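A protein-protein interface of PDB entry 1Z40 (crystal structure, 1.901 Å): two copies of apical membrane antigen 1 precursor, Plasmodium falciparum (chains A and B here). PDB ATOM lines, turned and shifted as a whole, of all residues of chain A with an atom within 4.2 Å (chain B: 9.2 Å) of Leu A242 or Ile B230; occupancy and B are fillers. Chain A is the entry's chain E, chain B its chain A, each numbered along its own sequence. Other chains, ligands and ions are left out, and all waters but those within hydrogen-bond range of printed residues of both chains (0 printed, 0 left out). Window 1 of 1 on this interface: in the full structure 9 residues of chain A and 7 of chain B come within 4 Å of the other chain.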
ATOM      1  N   ASN A 225     -33.309  -2.684 -12.399  1.00  0.00           N
ATOM      2  CA  ASN A 225     -33.109  -1.324 -12.863  1.00  0.00           C
ATOM      3  C   ASN A 225     -34.275  -0.987 -13.765  1.00  0.00           C
ATOM      4  O   ASN A 225     -34.609  -1.765 -14.640  1.00  0.00           O
ATOM      5  CB  ASN A 225     -31.841  -1.263 -13.729  1.00  0.00           C
ATOM      6  CG  ASN A 225     -30.567  -1.256 -12.891  1.00  0.00           C
ATOM      7  OD1 ASN A 225     -30.048  -2.307 -12.539  1.00  0.00           O
ATOM      8  ND2 ASN A 225     -30.098  -0.074 -12.545  1.00  0.00           N
ATOM      9  N   PHE A 227     -36.497   1.538 -16.446  1.00  0.00           N
ATOM     10  CA  PHE A 227     -36.452   2.536 -17.532  1.00  0.00           C
ATOM     11  C   PHE A 227     -37.816   2.860 -18.139  1.00  0.00           C
ATOM     12  O   PHE A 227     -38.644   1.964 -18.256  1.00  0.00           O
ATOM     13  CB  PHE A 227     -35.556   2.007 -18.656  1.00  0.00           C
ATOM     14  CG  PHE A 227     -34.188   1.653 -18.176  1.00  0.00           C
ATOM     15  CD1 PHE A 227     -33.221   2.659 -18.010  1.00  0.00           C
ATOM     16  CD2 PHE A 227     -33.901   0.351 -17.778  1.00  0.00           C
ATOM     17  CE1 PHE A 227     -31.974   2.356 -17.494  1.00  0.00           C
ATOM     18  CE2 PHE A 227     -32.623   0.030 -17.280  1.00  0.00           C
ATOM     19  CZ  PHE A 227     -31.682   1.028 -17.136  1.00  0.00           C
ATOM     20  N   LEU A 238     -34.415  -2.391 -25.389  1.00  0.00           N
ATOM     21  CA  LEU A 238     -33.487  -2.001 -24.314  1.00  0.00           C
ATOM     22  C   LEU A 238     -32.771  -3.187 -23.704  1.00  0.00           C
ATOM     23  O   LEU A 238     -31.535  -3.164 -23.524  1.00  0.00           O
ATOM     24  CB  LEU A 238     -34.212  -1.241 -23.194  1.00  0.00           C
ATOM     25  CG  LEU A 238     -34.553   0.210 -23.491  1.00  0.00           C
ATOM     26  CD1 LEU A 238     -35.631   0.747 -22.496  1.00  0.00           C
ATOM     27  CD2 LEU A 238     -33.274   1.089 -23.501  1.00  0.00           C
ATOM     28  N   VAL A 239     -33.551  -4.229 -23.420  1.00  0.00           N
ATOM     29  CA  VAL A 239     -33.033  -5.459 -22.847  1.00  0.00           C
ATOM     30  C   VAL A 239     -31.997  -6.017 -23.814  1.00  0.00           C
ATOM     31  O   VAL A 239     -30.904  -6.383 -23.397  1.00  0.00           O
ATOM     32  CB  VAL A 239     -34.140  -6.495 -22.612  1.00  0.00           C
ATOM     33  CG1 VAL A 239     -33.518  -7.858 -22.181  1.00  0.00           C
ATOM     34  CG2 VAL A 239     -35.109  -5.967 -21.489  1.00  0.00           C
ATOM     35  N   PHE A 240     -32.353  -6.038 -25.099  1.00  0.00           N
ATOM     36  CA  PHE A 240     -31.400  -6.480 -26.112  1.00  0.00           C
ATOM     37  C   PHE A 240     -30.082  -5.681 -26.078  1.00  0.00           C
ATOM     38  O   PHE A 240     -28.976  -6.258 -26.056  1.00  0.00           O
ATOM     39  CB  PHE A 240     -32.018  -6.405 -27.496  1.00  0.00           C
ATOM     40  CG  PHE A 240     -31.068  -6.889 -28.593  1.00  0.00           C
ATOM     41  CD1 PHE A 240     -30.867  -8.259 -28.771  1.00  0.00           C
ATOM     42  CD2 PHE A 240     -30.395  -5.985 -29.411  1.00  0.00           C
ATOM     43  CE1 PHE A 240     -29.986  -8.746 -29.775  1.00  0.00           C
ATOM     44  CE2 PHE A 240     -29.488  -6.474 -30.435  1.00  0.00           C
ATOM     45  CZ  PHE A 240     -29.314  -7.846 -30.602  1.00  0.00           C
ATOM     46  N   GLU A 241     -30.191  -4.355 -26.085  1.00  0.00           N
ATOM     47  CA  GLU A 241     -29.021  -3.458 -25.982  1.00  0.00           C
ATOM     48  C   GLU A 241     -28.097  -3.787 -24.799  1.00  0.00           C
ATOM     49  O   GLU A 241     -26.865  -3.728 -24.923  1.00  0.00           O
ATOM     50  CB  GLU A 241     -29.494  -2.003 -25.859  1.00  0.00           C
ATOM     51  CG  GLU A 241     -30.099  -1.477 -27.154  1.00  0.00           C
ATOM     52  CD  GLU A 241     -30.739  -0.088 -27.039  1.00  0.00           C
ATOM     53  OE1 GLU A 241     -31.071   0.375 -25.914  1.00  0.00           O
ATOM     54  OE2 GLU A 241     -30.938   0.548 -28.105  1.00  0.00           O
ATOM     55  N   LEU A 242     -28.698  -4.154 -23.670  1.00  0.00           N
ATOM     56  CA  LEU A 242     -27.959  -4.425 -22.431  1.00  0.00           C
ATOM     57  C   LEU A 242     -27.568  -5.891 -22.189  1.00  0.00           C
ATOM     58  O   LEU A 242     -26.940  -6.187 -21.167  1.00  0.00           O
ATOM     59  CB  LEU A 242     -28.830  -3.932 -21.248  1.00  0.00           C
ATOM     60  CG  LEU A 242     -29.029  -2.410 -21.247  1.00  0.00           C
ATOM     61  CD1 LEU A 242     -30.186  -2.045 -20.297  1.00  0.00           C
ATOM     62  CD2 LEU A 242     -27.697  -1.649 -20.872  1.00  0.00           C
ATOM     63  N   SER A 243     -27.978  -6.780 -23.100  1.00  0.00           N
ATOM     64  CA  SER A 243     -27.862  -8.230 -22.973  1.00  0.00           C
ATOM     65  C   SER A 243     -26.415  -8.754 -23.166  1.00  0.00           C
ATOM     66  O   SER A 243     -25.484  -7.966 -23.455  1.00  0.00           O
ATOM     67  CB  SER A 243     -28.835  -8.931 -23.915  1.00  0.00           C
ATOM     68  OG  SER A 243     -28.392  -8.925 -25.280  1.00  0.00           O
ATOM     69  N   TYR A 295     -27.516  -8.900 -18.858  1.00  0.00           N
ATOM     70  CA  TYR A 295     -28.833  -8.339 -18.507  1.00  0.00           C
ATOM     71  C   TYR A 295     -29.842  -8.776 -19.578  1.00  0.00           C
ATOM     72  O   TYR A 295     -30.189  -8.016 -20.503  1.00  0.00           O
ATOM     73  CB  TYR A 295     -28.697  -6.804 -18.350  1.00  0.00           C
ATOM     74  CG  TYR A 295     -28.048  -6.364 -17.046  1.00  0.00           C
ATOM     75  CD1 TYR A 295     -26.672  -6.153 -16.963  1.00  0.00           C
ATOM     76  CD2 TYR A 295     -28.826  -6.160 -15.868  1.00  0.00           C
ATOM     77  CE1 TYR A 295     -26.078  -5.753 -15.759  1.00  0.00           C
ATOM     78  CE2 TYR A 295     -28.230  -5.766 -14.673  1.00  0.00           C
ATOM     79  CZ  TYR A 295     -26.837  -5.587 -14.635  1.00  0.00           C
ATOM     80  OH  TYR A 295     -26.224  -5.206 -13.488  1.00  0.00           O
ATOM     81  N   ILE A 309     -35.239  -4.351 -15.658  1.00  0.00           N
ATOM     82  CA  ILE A 309     -34.203  -5.183 -16.345  1.00  0.00           C
ATOM     83  C   ILE A 309     -33.242  -5.786 -15.325  1.00  0.00           C
ATOM     84  O   ILE A 309     -32.885  -5.115 -14.369  1.00  0.00           O
ATOM     85  CB  ILE A 309     -33.485  -4.361 -17.448  1.00  0.00           C
ATOM     86  CG1 ILE A 309     -34.496  -3.835 -18.484  1.00  0.00           C
ATOM     87  CG2 ILE A 309     -32.397  -5.225 -18.187  1.00  0.00           C
ATOM     88  CD1 ILE A 309     -33.876  -2.957 -19.635  1.00  0.00           C
ATOM     89  N   PHE B 227     -19.451   1.998 -24.214  1.00  0.00           N
ATOM     90  CA  PHE B 227     -19.974   0.643 -23.910  1.00  0.00           C
ATOM     91  C   PHE B 227     -21.370   0.751 -23.321  1.00  0.00           C
ATOM     92  O   PHE B 227     -21.637   1.736 -22.648  1.00  0.00           O
ATOM     93  CB  PHE B 227     -19.099  -0.014 -22.838  1.00  0.00           C
ATOM     94  CG  PHE B 227     -17.645  -0.081 -23.214  1.00  0.00           C
ATOM     95  CD1 PHE B 227     -16.761   0.919 -22.822  1.00  0.00           C
ATOM     96  CD2 PHE B 227     -17.174  -1.121 -24.002  1.00  0.00           C
ATOM     97  CE1 PHE B 227     -15.398   0.859 -23.193  1.00  0.00           C
ATOM     98  CE2 PHE B 227     -15.823  -1.163 -24.377  1.00  0.00           C
ATOM     99  CZ  PHE B 227     -14.961  -0.172 -23.965  1.00  0.00           C
ATOM    100  N   PRO B 228     -22.226  -0.254 -23.550  1.00  0.00           N
ATOM    101  CA  PRO B 228     -23.501  -0.310 -22.781  1.00  0.00           C
ATOM    102  C   PRO B 228     -23.264  -0.479 -21.283  1.00  0.00           C
ATOM    103  O   PRO B 228     -22.353  -1.219 -20.867  1.00  0.00           O
ATOM    104  CB  PRO B 228     -24.184  -1.561 -23.345  1.00  0.00           C
ATOM    105  CG  PRO B 228     -23.573  -1.762 -24.733  1.00  0.00           C
ATOM    106  CD  PRO B 228     -22.110  -1.384 -24.499  1.00  0.00           C
ATOM    107  N   ALA B 229     -24.057   0.227 -20.453  1.00  0.00           N
ATOM    108  CA  ALA B 229     -23.902   0.170 -18.984  1.00  0.00           C
ATOM    109  C   ALA B 229     -25.310   0.483 -18.448  1.00  0.00           C
ATOM    110  O   ALA B 229     -25.881   1.526 -18.759  1.00  0.00           O
ATOM    111  CB  ALA B 229     -22.855   1.195 -18.445  1.00  0.00           C
ATOM    112  N   ILE B 230     -25.905  -0.479 -17.759  1.00  0.00           N
ATOM    113  CA  ILE B 230     -27.292  -0.336 -17.279  1.00  0.00           C
ATOM    114  C   ILE B 230     -27.427   0.754 -16.209  1.00  0.00           C
ATOM    115  O   ILE B 230     -28.513   1.348 -16.058  1.00  0.00           O
ATOM    116  CB  ILE B 230     -27.857  -1.688 -16.743  1.00  0.00           C
ATOM    117  CG1 ILE B 230     -29.368  -1.616 -16.530  1.00  0.00           C
ATOM    118  CG2 ILE B 230     -27.111  -2.132 -15.449  1.00  0.00           C
ATOM    119  CD1 ILE B 230     -30.031  -2.963 -16.404  1.00  0.00           C
ATOM    120  N   ASP B 231     -26.372   1.001 -15.459  1.00  0.00           N
ATOM    121  CA  ASP B 231     -26.424   2.037 -14.408  1.00  0.00           C
ATOM    122  C   ASP B 231     -25.076   2.598 -14.089  1.00  0.00           C
ATOM    123  O   ASP B 231     -24.045   2.140 -14.633  1.00  0.00           O
ATOM    124  CB  ASP B 231     -27.184   1.575 -13.139  1.00  0.00           C
ATOM    125  CG  ASP B 231     -26.535   0.389 -12.425  1.00  0.00           C
ATOM    126  OD1 ASP B 231     -25.384  -0.012 -12.729  1.00  0.00           O
ATOM    127  OD2 ASP B 231     -27.233  -0.208 -11.572  1.00  0.00           O
ATOM    128  N   LEU B 232     -25.044   3.579 -13.197  1.00  0.00           N
ATOM    129  CA  LEU B 232     -23.744   4.139 -12.806  1.00  0.00           C
ATOM    130  C   LEU B 232     -22.825   3.076 -12.204  1.00  0.00           C
ATOM    131  O   LEU B 232     -21.612   3.087 -12.488  1.00  0.00           O
ATOM    132  CB  LEU B 232     -23.962   5.274 -11.796  1.00  0.00           C
ATOM    133  CG  LEU B 232     -22.734   5.903 -11.149  1.00  0.00           C
ATOM    134  CD1 LEU B 232     -21.802   6.525 -12.202  1.00  0.00           C
ATOM    135  CD2 LEU B 232     -23.197   6.962 -10.101  1.00  0.00           C
ATOM    136  N   PHE B 233     -23.381   2.155 -11.400  1.00  0.00           N
ATOM    137  CA  PHE B 233     -22.505   1.103 -10.805  1.00  0.00           C
ATOM    138  C   PHE B 233     -21.799   0.309 -11.897  1.00  0.00           C
ATOM    139  O   PHE B 233     -20.593   0.051 -11.824  1.00  0.00           O
ATOM    140  CB  PHE B 233     -23.342   0.132  -9.964  1.00  0.00           C
ATOM    141  CG  PHE B 233     -22.579  -0.503  -8.816  1.00  0.00           C
ATOM    142  CD1 PHE B 233     -23.046  -0.363  -7.503  1.00  0.00           C
ATOM    143  CD2 PHE B 233     -21.449  -1.280  -9.044  1.00  0.00           C
ATOM    144  CE1 PHE B 233     -22.367  -0.953  -6.423  1.00  0.00           C
ATOM    145  CE2 PHE B 233     -20.757  -1.877  -7.981  1.00  0.00           C
ATOM    146  CZ  PHE B 233     -21.213  -1.704  -6.667  1.00  0.00           C
ATOM    147  N   GLU B 234     -22.558  -0.096 -12.909  1.00  0.00           N
ATOM    148  CA  GLU B 234     -21.966  -0.854 -14.019  1.00  0.00           C
ATOM    149  C   GLU B 234     -20.908  -0.066 -14.781  1.00  0.00           C
ATOM    150  O   GLU B 234     -19.867  -0.628 -15.135  1.00  0.00           O
ATOM    151  CB  GLU B 234     -23.035  -1.384 -14.964  1.00  0.00           C
ATOM    152  CG  GLU B 234     -23.801  -2.610 -14.431  1.00  0.00           C
ATOM    153  CD  GLU B 234     -22.876  -3.760 -14.002  1.00  0.00           C
ATOM    154  OE1 GLU B 234     -21.977  -4.148 -14.777  1.00  0.00           O
ATOM    155  OE2 GLU B 234     -23.071  -4.291 -12.888  1.00  0.00           O
ATOM    156  N   CYS B 235     -21.174   1.216 -15.050  1.00  0.00           N
ATOM    157  CA  CYS B 235     -20.168   2.091 -15.653  1.00  0.00           C
ATOM    158  C   CYS B 235     -18.890   2.160 -14.809  1.00  0.00           C
ATOM    159  O   CYS B 235     -17.783   1.928 -15.319  1.00  0.00           O
ATOM    160  CB  CYS B 235     -20.706   3.512 -15.880  1.00  0.00           C
ATOM    161  SG  CYS B 235     -19.552   4.633 -16.807  1.00  0.00           S
ATOM    162  N   ASN B 236     -19.041   2.464 -13.523  1.00  0.00           N
ATOM    163  CA  ASN B 236     -17.910   2.496 -12.600  1.00  0.00           C
ATOM    164  C   ASN B 236     -17.150   1.174 -12.602  1.00  0.00           C
ATOM    165  O   ASN B 236     -15.894   1.182 -12.609  1.00  0.00           O
ATOM    166  CB  ASN B 236     -18.346   2.882 -11.181  1.00  0.00           C
ATOM    167  CG  ASN B 236     -17.151   3.157 -10.266  1.00  0.00           C
ATOM    168  OD1 ASN B 236     -16.704   2.276  -9.534  1.00  0.00           O
ATOM    169  ND2 ASN B 236     -16.622   4.369 -10.330  1.00  0.00           N
ATOM    170  N   LYS B 237     -17.875   0.056 -12.628  1.00  0.00           N
ATOM    171  CA  LYS B 237     -17.193  -1.252 -12.721  1.00  0.00           C
ATOM    172  C   LYS B 237     -16.334  -1.361 -13.983  1.00  0.00           C
ATOM    173  O   LYS B 237     -15.213  -1.906 -13.938  1.00  0.00           O
ATOM    174  CB  LYS B 237     -18.197  -2.397 -12.770  1.00  0.00           C
ATOM    175  CG  LYS B 237     -18.846  -2.858 -11.486  1.00  0.00           C
ATOM    176  CD  LYS B 237     -19.530  -4.258 -11.804  1.00  0.00           C
ATOM    177  CE  LYS B 237     -20.487  -4.680 -10.704  1.00  0.00           C
ATOM    178  NZ  LYS B 237     -21.305  -5.886 -11.086  1.00  0.00           N
ATOM    179  N   LEU B 238     -16.882  -0.925 -15.122  1.00  0.00           N
ATOM    180  CA  LEU B 238     -16.168  -1.019 -16.396  1.00  0.00           C
ATOM    181  C   LEU B 238     -14.919  -0.140 -16.437  1.00  0.00           C
ATOM    182  O   LEU B 238     -13.858  -0.553 -16.950  1.00  0.00           O
ATOM    183  CB  LEU B 238     -17.059  -0.644 -17.572  1.00  0.00           C
ATOM    184  CG  LEU B 238     -18.230  -1.584 -17.834  1.00  0.00           C
ATOM    185  CD1 LEU B 238     -19.191  -0.951 -18.813  1.00  0.00           C
ATOM    186  CD2 LEU B 238     -17.712  -2.917 -18.348  1.00  0.00           C
ATOM    187  N   TYR B 300     -20.799   8.752 -17.795  1.00  0.00           N
ATOM    188  CA  TYR B 300     -21.948   7.879 -17.950  1.00  0.00           C
ATOM    189  C   TYR B 300     -23.180   8.662 -18.398  1.00  0.00           C
ATOM    190  O   TYR B 300     -23.653   9.559 -17.667  1.00  0.00           O
ATOM    191  CB  TYR B 300     -22.271   7.179 -16.623  1.00  0.00           C
ATOM    192  CG  TYR B 300     -23.425   6.253 -16.774  1.00  0.00           C
ATOM    193  CD1 TYR B 300     -23.391   5.223 -17.727  1.00  0.00           C
ATOM    194  CD2 TYR B 300     -24.571   6.412 -16.006  1.00  0.00           C
ATOM    195  CE1 TYR B 300     -24.473   4.391 -17.901  1.00  0.00           C
ATOM    196  CE2 TYR B 300     -25.653   5.581 -16.153  1.00  0.00           C
ATOM    197  CZ  TYR B 300     -25.602   4.551 -17.089  1.00  0.00           C
ATOM    198  OH  TYR B 300     -26.718   3.746 -17.255  1.00  0.00           O
ATOM    199  N   ASN B 301     -23.695   8.318 -19.580  1.00  0.00           N
ATOM    200  CA  ASN B 301     -24.930   8.907 -20.069  1.00  0.00           C
ATOM    201  C   ASN B 301     -26.127   8.111 -19.553  1.00  0.00           C
ATOM    202  O   ASN B 301     -26.405   7.011 -20.013  1.00  0.00           O
ATOM    203  CB  ASN B 301     -24.940   8.993 -21.613  1.00  0.00           C
ATOM    204  CG  ASN B 301     -26.131   9.775 -22.144  1.00  0.00           C
ATOM    205  OD1 ASN B 301     -27.238   9.633 -21.639  1.00  0.00           O
ATOM    206  ND2 ASN B 301     -25.917  10.576 -23.194  1.00  0.00           N
ATOM    207  N   THR B 302     -26.855   8.691 -18.606  1.00  0.00           N
ATOM    208  CA  THR B 302     -27.986   8.021 -17.967  1.00  0.00           C
ATOM    209  C   THR B 302     -29.210   7.888 -18.880  1.00  0.00           C
ATOM    210  O   THR B 302     -30.153   7.167 -18.552  1.00  0.00           O
ATOM    211  CB  THR B 302     -28.436   8.816 -16.732  1.00  0.00           C
ATOM    212  OG1 THR B 302     -28.805  10.130 -17.166  1.00  0.00           O
ATOM    213  CG2 THR B 302     -27.306   8.920 -15.731  1.00  0.00           C
ATOM    214  N   GLU B 303     -29.242   8.623 -19.986  1.00  0.00           N
ATOM    215  CA  GLU B 303     -30.416   8.612 -20.859  1.00  0.00           C
ATOM    216  C   GLU B 303     -30.274   7.590 -21.949  1.00  0.00           C
ATOM    217  O   GLU B 303     -31.276   7.089 -22.454  1.00  0.00           O
ATOM    218  CB  GLU B 303     -30.700   9.990 -21.464  1.00  0.00           C
ATOM    219  CG  GLU B 303     -30.605  11.058 -20.410  1.00  0.00           C
ATOM    220  CD  GLU B 303     -31.723  12.029 -20.405  1.00  0.00           C
ATOM    221  OE1 GLU B 303     -31.404  13.222 -20.209  1.00  0.00           O
ATOM    222  OE2 GLU B 303     -32.910  11.624 -20.552  1.00  0.00           O
ATOM    223  N   THR B 304     -29.028   7.282 -22.288  1.00  0.00           N
ATOM    224  CA  THR B 304     -28.738   6.315 -23.364  1.00  0.00           C
ATOM    225  C   THR B 304     -28.062   5.047 -22.817  1.00  0.00           C
ATOM    226  O   THR B 304     -27.848   4.100 -23.562  1.00  0.00           O
ATOM    227  CB  THR B 304     -27.829   6.937 -24.441  1.00  0.00           C
ATOM    228  OG1 THR B 304     -26.590   7.322 -23.843  1.00  0.00           O
ATOM    229  CG2 THR B 304     -28.505   8.145 -25.095  1.00  0.00           C
ATOM    230  N   GLN B 305     -27.736   5.038 -21.525  1.00  0.00           N
ATOM    231  CA  GLN B 305     -27.118   3.878 -20.858  1.00  0.00           C
ATOM    232  C   GLN B 305     -25.831   3.527 -21.571  1.00  0.00           C
ATOM    233  O   GLN B 305     -25.658   2.399 -22.010  1.00  0.00           O
ATOM    234  CB  GLN B 305     -28.047   2.649 -20.872  1.00  0.00           C
ATOM    235  CG  GLN B 305     -29.331   2.823 -20.024  1.00  0.00           C
ATOM    236  CD  GLN B 305     -30.429   3.563 -20.761  1.00  0.00           C
ATOM    237  OE1 GLN B 305     -31.078   4.460 -20.202  1.00  0.00           O
ATOM    238  NE2 GLN B 305     -30.657   3.194 -22.016  1.00  0.00           N
ATOM    239  N   LYS B 306     -24.950   4.518 -21.664  1.00  0.00           N
ATOM    240  CA  LYS B 306     -23.669   4.377 -22.320  1.00  0.00           C
ATOM    241  C   LYS B 306     -22.624   4.924 -21.391  1.00  0.00           C
ATOM    242  O   LYS B 306     -22.810   5.985 -20.783  1.00  0.00           O
ATOM    243  CB  LYS B 306     -23.625   5.111 -23.667  1.00  0.00           C
ATOM    244  CG  LYS B 306     -24.518   4.540 -24.769  1.00  0.00           C
ATOM    245  CD  LYS B 306     -24.106   3.138 -25.237  1.00  0.00           C
ATOM    246  CE  LYS B 306     -24.849   2.758 -26.545  1.00  0.00           C
ATOM    247  NZ  LYS B 306     -26.330   2.945 -26.421  1.00  0.00           N
ATOM    248  N   CYS B 307     -21.538   4.166 -21.261  1.00  0.00           N
ATOM    249  CA  CYS B 307     -20.408   4.504 -20.423  1.00  0.00           C
ATOM    250  C   CYS B 307     -19.292   4.900 -21.402  1.00  0.00           C
ATOM    251  O   CYS B 307     -18.915   4.078 -22.279  1.00  0.00           O
ATOM    252  CB  CYS B 307     -20.014   3.265 -19.588  1.00  0.00           C
ATOM    253  SG  CYS B 307     -18.711   3.484 -18.331  1.00  0.00           S
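The side-chain carboxylate (OD2) of Asp B231 lies within hydrogen-bond range of the side-chain amide nitrogen (ND2) of Asn A225 (3.0 Å). The side-chain carboxylate of Glu B234 sits at hydrogen-bond distance from the side-chain hydroxyl of Tyr A295 (3.3 Å).
The backbone carbonyl oxygen of Gln B305 is in hydrogen-bond range of the backbone NH of Ala B229 (3.1 Å). The side-chain carboxylate (OD1) of Asp B231 sits at hydrogen-bond distance from the backbone NH (N) of Glu B234 (2.8 Å). The side-chain hydroxyl of Tyr B300 is in hydrogen-bond range of the backbone NH of Asp B231. The backbone carbonyl oxygen (O) of Thr B302 sits close to the side-chain amide oxygen (OE1) of Gln B305 (3.3 Å). O of Glu B303 sits close to OE1 of Gln B305 (3.5 Å). The backbone NH (N) of Ile A309 sits at hydrogen-bond distance from the backbone carbonyl oxygen (O) of Asn A225, at 2.8 Å.
CD1 of Ile B230 touches CB of Asn A225, 3.6 Å away. Ile B230 touches Phe A227. Phe A227 touches Gln B305 (CE1 to OE1, 3.5 Å). Leu A238 touches Gln B305. Pro B228 touches Glu A241. CD2 of Leu A242 touches N of Ile B230 (3.8 Å). CD2 of Tyr A295 touches CD1 of Ile B230, 3.5 Å away. Ile A309 touches Ile B230 (CG2 to CD1, 3.7 Å).
Printed residues of chain B within 4 Å of Leu A242: Ile B230 (3.8 Å). Ile B230 touches five residues of chain A. Of chain B, only Ile B230 (3.5 Å) and Glu B234 (3.3 Å) come within 4 Å of Tyr A295. Of the printed residues of chain A, Gln B305 touches Phe A227 and Leu A238. Of the printed residues of chain B, Ile A309 touches Ile B230. Printed residues of chain B within 4 Å of Glu A241: Pro B228. Of the printed residues of chain B, Phe A227 touches Ile B230 (3.4 Å) and Gln B305 (3.5 Å). Tyr B300 touches none of the printed residues of chain A. Thr B302 touches none of the printed residues of chain A. The nearest printed residue of chain B that does not touch Leu A242 is Ala B229 (4.01 Å). The nearest printed residue of chain A that does not touch Pro B228 is Leu A242 (4.3 Å).
Of the 20 printed residues of chain B, 5 touch a printed residue of chain A. Hydrophobic or aromatic side chains of chain B that line the printed part of chain A: Pro B228 and Ile B230. Hydrophobic or aromatic side chains of chain A within 4 Å of the printed part of chain B: Phe A227, Leu A238, Leu A242, Tyr A295 and Ile A309. Among the printed residues, no Asp or Glu carboxylate lies within 4 Å of a Lys or Arg side-chain nitrogen of the other chain.
Positions printed for both chains: 227 and 238.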
